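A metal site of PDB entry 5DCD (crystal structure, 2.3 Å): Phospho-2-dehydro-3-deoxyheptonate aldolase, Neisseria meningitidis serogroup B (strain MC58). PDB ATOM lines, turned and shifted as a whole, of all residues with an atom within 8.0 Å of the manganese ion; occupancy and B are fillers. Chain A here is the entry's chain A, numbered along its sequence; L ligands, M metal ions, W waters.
NZ of Lys 99 is in salt-bridge range of OD1 of Asp 324, 3.4 Å away.
NH1 of Arg 94 sits at hydrogen-bond distance from SD of Met 302, at 3.5 Å.
The backbone carbonyl oxygen (O) of Pro 62 sits at hydrogen-bond distance from the guanidinium group (NE) of Arg 94 (2.8 Å).
The side-chain carboxylate of Glu 304 lies within hydrogen-bond range of the side-chain hydroxyl of Ser 269 (2.7 Å).
The backbone carbonyl oxygen (O) of Cys 63 is in hydrogen-bond range of the guanidinium group (NH2) of Arg 94, at 2.9 Å.
N of Cys 63 is in hydrogen-bond range of SG of Cys 326.
SG of Cys 63 lies close to OG1 of Thr 323 (2.9 Å).
ND1 of His 270 lies within hydrogen-bond range of OD2 of Asp 267 (2.7 Å).
Residues that only touch the manganese ion: Arg 94.
The manganese ion is bound by OE2 of Glu 304 (2.0 Å), water W1 (2.0 Å), OD2 of Asp 324 (2.0 Å), NE2 of His 270 (2.4 Å) and SG of Cys 63 (2.6 Å).
The manganese ion has five donor atoms within binding distance.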
ATOM      1  N   GLY A  61       1.035 -31.275  -2.589  1.00  0.00           N
ATOM      2  CA  GLY A  61      -0.363 -31.288  -2.229  1.00  0.00           C
ATOM      3  C   GLY A  61      -0.883 -29.874  -2.059  1.00  0.00           C
ATOM      4  O   GLY A  61      -0.173 -28.908  -2.319  1.00  0.00           O
ATOM      5  N   PRO A  62      -2.138 -29.740  -1.620  1.00  0.00           N
ATOM      6  CA  PRO A  62      -2.780 -28.446  -1.343  1.00  0.00           C
ATOM      7  C   PRO A  62      -1.976 -27.460  -0.473  1.00  0.00           C
ATOM      8  O   PRO A  62      -1.183 -27.879   0.374  1.00  0.00           O
ATOM      9  CB  PRO A  62      -4.061 -28.869  -0.602  1.00  0.00           C
ATOM     10  CG  PRO A  62      -4.410 -30.207  -1.198  1.00  0.00           C
ATOM     11  CD  PRO A  62      -3.071 -30.879  -1.421  1.00  0.00           C
ATOM     12  N   CYS A  63      -2.189 -26.148  -0.646  1.00  0.00           N
ATOM     13  CA  CYS A  63      -1.598 -25.175   0.289  1.00  0.00           C
ATOM     14  C   CYS A  63      -2.148 -25.432   1.715  1.00  0.00           C
ATOM     15  O   CYS A  63      -1.381 -25.494   2.662  1.00  0.00           O
ATOM     16  CB  CYS A  63      -1.899 -23.735  -0.158  1.00  0.00           C
ATOM     17  SG  CYS A  63      -1.416 -22.445   1.039  1.00  0.00           S
ATOM     18  N   SER A  64      -3.447 -25.585   1.844  1.00  0.00           N
ATOM     19  CA  SER A  64      -4.072 -25.940   3.132  1.00  0.00           C
ATOM     20  C   SER A  64      -5.196 -26.925   2.902  1.00  0.00           C
ATOM     21  O   SER A  64      -5.915 -26.819   1.903  1.00  0.00           O
ATOM     22  CB  SER A  64      -4.652 -24.711   3.815  1.00  0.00           C
ATOM     23  OG  SER A  64      -5.670 -24.127   3.017  1.00  0.00           O
ATOM     24  N   ARG A  94       1.419 -33.309   0.972  1.00  0.00           N
ATOM     25  CA  ARG A  94       1.357 -32.148   1.817  1.00  0.00           C
ATOM     26  C   ARG A  94       0.012 -32.137   2.529  1.00  0.00           C
ATOM     27  O   ARG A  94      -1.023 -32.036   1.880  1.00  0.00           O
ATOM     28  CB  ARG A  94       1.393 -30.934   0.943  1.00  0.00           C
ATOM     29  CG  ARG A  94       2.433 -29.903   1.244  1.00  0.00           C
ATOM     30  CD  ARG A  94       2.253 -28.709   0.298  1.00  0.00           C
ATOM     31  NE  ARG A  94       1.577 -27.622   0.967  1.00  0.00           N
ATOM     32  CZ  ARG A  94       2.182 -26.566   1.490  1.00  0.00           C
ATOM     33  NH1 ARG A  94       3.506 -26.431   1.402  1.00  0.00           N
ATOM     34  NH2 ARG A  94       1.472 -25.628   2.079  1.00  0.00           N
ATOM     35  N   TYR A  96      -1.134 -29.748   5.131  1.00  0.00           N
ATOM     36  CA  TYR A  96      -1.013 -28.572   5.969  1.00  0.00           C
ATOM     37  C   TYR A  96      -2.398 -28.139   6.381  1.00  0.00           C
ATOM     38  O   TYR A  96      -3.284 -28.017   5.540  1.00  0.00           O
ATOM     39  CB  TYR A  96      -0.339 -27.425   5.225  1.00  0.00           C
ATOM     40  CG  TYR A  96       1.165 -27.534   5.085  1.00  0.00           C
ATOM     41  CD1 TYR A  96       1.784 -28.753   4.812  1.00  0.00           C
ATOM     42  CD2 TYR A  96       1.975 -26.393   5.179  1.00  0.00           C
ATOM     43  CE1 TYR A  96       3.167 -28.827   4.657  1.00  0.00           C
ATOM     44  CE2 TYR A  96       3.334 -26.469   5.014  1.00  0.00           C
ATOM     45  CZ  TYR A  96       3.932 -27.670   4.747  1.00  0.00           C
ATOM     46  OH  TYR A  96       5.305 -27.722   4.598  1.00  0.00           O
ATOM     47  N   GLU A  98      -3.158 -25.269   8.100  1.00  0.00           N
ATOM     48  CA  GLU A  98      -3.271 -23.808   8.224  1.00  0.00           C
ATOM     49  C   GLU A  98      -2.185 -23.060   7.444  1.00  0.00           C
ATOM     50  O   GLU A  98      -1.019 -23.469   7.428  1.00  0.00           O
ATOM     51  CB  GLU A  98      -3.152 -23.432   9.702  1.00  0.00           C
ATOM     52  CG  GLU A  98      -3.431 -21.970  10.029  1.00  0.00           C
ATOM     53  CD  GLU A  98      -3.311 -21.669  11.524  1.00  0.00           C
ATOM     54  OE1 GLU A  98      -3.439 -20.496  11.930  1.00  0.00           O
ATOM     55  OE2 GLU A  98      -3.090 -22.646  12.290  1.00  0.00           O
ATOM     56  N   LYS A  99      -2.592 -21.969   6.784  1.00  0.00           N
ATOM     57  CA  LYS A  99      -1.630 -20.992   6.295  1.00  0.00           C
ATOM     58  C   LYS A  99      -1.542 -19.827   7.288  1.00  0.00           C
ATOM     59  O   LYS A  99      -2.487 -19.032   7.391  1.00  0.00           O
ATOM     60  CB  LYS A  99      -1.998 -20.447   4.905  1.00  0.00           C
ATOM     61  CG  LYS A  99      -1.091 -19.306   4.486  1.00  0.00           C
ATOM     62  CD  LYS A  99      -1.202 -18.911   3.021  1.00  0.00           C
ATOM     63  CE  LYS A  99      -0.224 -17.784   2.709  1.00  0.00           C
ATOM     64  NZ  LYS A  99       1.192 -18.258   2.582  1.00  0.00           N
ATOM     65  N   PRO A 100      -0.381 -19.687   7.981  1.00  0.00           N
ATOM     66  CA  PRO A 100      -0.176 -18.509   8.820  1.00  0.00           C
ATOM     67  C   PRO A 100      -0.395 -17.234   8.052  1.00  0.00           C
ATOM     68  O   PRO A 100       0.112 -17.097   6.935  1.00  0.00           O
ATOM     69  CB  PRO A 100       1.299 -18.607   9.252  1.00  0.00           C
ATOM     70  CG  PRO A 100       1.856 -19.845   8.647  1.00  0.00           C
ATOM     71  CD  PRO A 100       0.720 -20.667   8.122  1.00  0.00           C
ATOM     72  N   GLU A 145       3.118 -28.782   8.505  1.00  0.00           N
ATOM     73  CA  GLU A 145       3.838 -27.721   9.210  1.00  0.00           C
ATOM     74  C   GLU A 145       3.365 -27.639  10.655  1.00  0.00           C
ATOM     75  O   GLU A 145       2.172 -27.545  10.956  1.00  0.00           O
ATOM     76  CB  GLU A 145       3.677 -26.352   8.563  1.00  0.00           C
ATOM     77  CG  GLU A 145       4.539 -25.321   9.275  1.00  0.00           C
ATOM     78  CD  GLU A 145       4.411 -23.884   8.765  1.00  0.00           C
ATOM     79  OE1 GLU A 145       3.798 -23.649   7.717  1.00  0.00           O
ATOM     80  OE2 GLU A 145       4.942 -22.963   9.444  1.00  0.00           O
ATOM     81  N   LYS A 188      12.661 -23.453   6.394  1.00  0.00           N
ATOM     82  CA  LYS A 188      12.708 -22.462   5.314  1.00  0.00           C
ATOM     83  C   LYS A 188      13.572 -21.259   5.613  1.00  0.00           C
ATOM     84  O   LYS A 188      13.621 -20.774   6.735  1.00  0.00           O
ATOM     85  CB  LYS A 188      11.318 -21.974   4.999  1.00  0.00           C
ATOM     86  CG  LYS A 188      10.396 -23.129   4.680  1.00  0.00           C
ATOM     87  CD  LYS A 188       9.110 -22.674   4.051  1.00  0.00           C
ATOM     88  CE  LYS A 188       8.705 -23.686   2.993  1.00  0.00           C
ATOM     89  NZ  LYS A 188       7.686 -23.215   2.034  1.00  0.00           N
ATOM     90  N   ASP A 267      11.479 -25.225  -2.956  1.00  0.00           N
ATOM     91  CA  ASP A 267      10.046 -25.015  -3.019  1.00  0.00           C
ATOM     92  C   ASP A 267       9.766 -24.319  -4.347  1.00  0.00           C
ATOM     93  O   ASP A 267      10.260 -23.230  -4.578  1.00  0.00           O
ATOM     94  CB  ASP A 267       9.632 -24.134  -1.844  1.00  0.00           C
ATOM     95  CG  ASP A 267       8.143 -23.919  -1.747  1.00  0.00           C
ATOM     96  OD1 ASP A 267       7.373 -24.368  -2.617  1.00  0.00           O
ATOM     97  OD2 ASP A 267       7.739 -23.258  -0.794  1.00  0.00           O
ATOM     98  N   SER A 269       6.948 -23.167  -5.197  1.00  0.00           N
ATOM     99  CA  SER A 269       5.882 -22.220  -4.917  1.00  0.00           C
ATOM    100  C   SER A 269       6.354 -21.044  -4.098  1.00  0.00           C
ATOM    101  O   SER A 269       7.544 -20.747  -4.024  1.00  0.00           O
ATOM    102  CB  SER A 269       4.729 -22.925  -4.211  1.00  0.00           C
ATOM    103  OG  SER A 269       3.500 -22.285  -4.501  1.00  0.00           O
ATOM    104  N   HIS A 270       5.383 -20.365  -3.493  1.00  0.00           N
ATOM    105  CA  HIS A 270       5.636 -19.210  -2.646  1.00  0.00           C
ATOM    106  C   HIS A 270       6.470 -18.108  -3.305  1.00  0.00           C
ATOM    107  O   HIS A 270       6.011 -17.572  -4.308  1.00  0.00           O
ATOM    108  CB  HIS A 270       6.182 -19.678  -1.329  1.00  0.00           C
ATOM    109  CG  HIS A 270       5.228 -20.573  -0.626  1.00  0.00           C
ATOM    110  ND1 HIS A 270       5.458 -21.929  -0.462  1.00  0.00           N
ATOM    111  CD2 HIS A 270       3.996 -20.338  -0.119  1.00  0.00           C
ATOM    112  CE1 HIS A 270       4.417 -22.469   0.141  1.00  0.00           C
ATOM    113  NE2 HIS A 270       3.524 -21.525   0.358  1.00  0.00           N
ATOM    114  N   MET A 302       9.268 -28.963  -3.295  1.00  0.00           N
ATOM    115  CA  MET A 302       7.932 -28.785  -2.738  1.00  0.00           C
ATOM    116  C   MET A 302       7.035 -28.176  -3.818  1.00  0.00           C
ATOM    117  O   MET A 302       7.483 -27.344  -4.595  1.00  0.00           O
ATOM    118  CB  MET A 302       8.011 -27.871  -1.516  1.00  0.00           C
ATOM    119  CG  MET A 302       6.694 -27.666  -0.822  1.00  0.00           C
ATOM    120  SD  MET A 302       6.896 -26.717   0.710  1.00  0.00           S
ATOM    121  CE  MET A 302       7.849 -27.826   1.738  1.00  0.00           C
ATOM    122  N   GLU A 304       2.830 -26.902  -4.681  1.00  0.00           N
ATOM    123  CA  GLU A 304       1.507 -26.634  -4.199  1.00  0.00           C
ATOM    124  C   GLU A 304       0.526 -27.003  -5.284  1.00  0.00           C
ATOM    125  O   GLU A 304       0.504 -26.383  -6.330  1.00  0.00           O
ATOM    126  CB  GLU A 304       1.372 -25.190  -3.715  1.00  0.00           C
ATOM    127  CG  GLU A 304       1.887 -25.004  -2.294  1.00  0.00           C
ATOM    128  CD  GLU A 304       1.642 -23.619  -1.736  1.00  0.00           C
ATOM    129  OE1 GLU A 304       1.795 -22.618  -2.467  1.00  0.00           O
ATOM    130  OE2 GLU A 304       1.313 -23.526  -0.548  1.00  0.00           O
ATOM    131  N   SER A 321      -8.167 -24.554  -3.825  1.00  0.00           N
ATOM    132  CA  SER A 321      -7.602 -23.915  -2.621  1.00  0.00           C
ATOM    133  C   SER A 321      -8.348 -22.676  -2.117  1.00  0.00           C
ATOM    134  O   SER A 321      -8.860 -21.868  -2.901  1.00  0.00           O
ATOM    135  CB  SER A 321      -6.156 -23.573  -2.859  1.00  0.00           C
ATOM    136  OG  SER A 321      -5.569 -23.054  -1.701  1.00  0.00           O
ATOM    137  N   THR A 323      -6.594 -20.988   0.389  1.00  0.00           N
ATOM    138  CA  THR A 323      -5.402 -20.213   0.740  1.00  0.00           C
ATOM    139  C   THR A 323      -4.617 -19.855  -0.537  1.00  0.00           C
ATOM    140  O   THR A 323      -5.191 -19.187  -1.386  1.00  0.00           O
ATOM    141  CB  THR A 323      -4.588 -20.898   1.834  1.00  0.00           C
ATOM    142  OG1 THR A 323      -4.253 -22.224   1.417  1.00  0.00           O
ATOM    143  CG2 THR A 323      -5.448 -20.955   3.113  1.00  0.00           C
ATOM    144  N   ASP A 324      -3.345 -20.260  -0.689  1.00  0.00           N
ATOM    145  CA  ASP A 324      -2.556 -19.886  -1.887  1.00  0.00           C
ATOM    146  C   ASP A 324      -3.052 -20.676  -3.120  1.00  0.00           C
ATOM    147  O   ASP A 324      -3.602 -21.790  -2.993  1.00  0.00           O
ATOM    148  CB  ASP A 324      -1.049 -20.191  -1.743  1.00  0.00           C
ATOM    149  CG  ASP A 324      -0.389 -19.490  -0.568  1.00  0.00           C
ATOM    150  OD1 ASP A 324      -0.771 -18.340  -0.229  1.00  0.00           O
ATOM    151  OD2 ASP A 324       0.562 -20.107  -0.004  1.00  0.00           O
ATOM    152  N   ALA A 325      -2.851 -20.092  -4.294  1.00  0.00           N
ATOM    153  CA  ALA A 325      -3.284 -20.739  -5.534  1.00  0.00           C
ATOM    154  C   ALA A 325      -2.387 -21.932  -5.829  1.00  0.00           C
ATOM    155  O   ALA A 325      -1.164 -21.852  -5.644  1.00  0.00           O
ATOM    156  CB  ALA A 325      -3.281 -19.746  -6.720  1.00  0.00           C
ATOM    157  N   CYS A 326      -2.992 -23.036  -6.278  1.00  0.00           N
ATOM    158  CA  CYS A 326      -2.271 -24.265  -6.588  1.00  0.00           C
ATOM    159  C   CYS A 326      -2.358 -24.589  -8.061  1.00  0.00           C
ATOM    160  O   CYS A 326      -3.219 -24.055  -8.733  1.00  0.00           O
ATOM    161  CB  CYS A 326      -2.853 -25.405  -5.789  1.00  0.00           C
ATOM    162  SG  CYS A 326      -2.696 -25.140  -4.004  1.00  0.00           S
HETATM  163  C1  LIG L   1       5.103 -21.202   3.399  1.00  0.00           C
HETATM  164  N1  LIG L   1       6.162 -20.262   3.794  1.00  0.00           N
HETATM  165  C2  LIG L   1       7.135 -20.158   2.710  1.00  0.00           C
HETATM  166  C3  LIG L   1       5.605 -18.921   3.868  1.00  0.00           C
HETATM  167  O1  LIG L   1       6.615 -20.597   4.950  1.00  0.00           O
HETATM  168 MN    MN M   1       1.128 -21.952   0.601  1.00  0.00          MN
HETATM  169  O   HOH W   1       1.391 -21.460   2.542  1.00  0.00           O
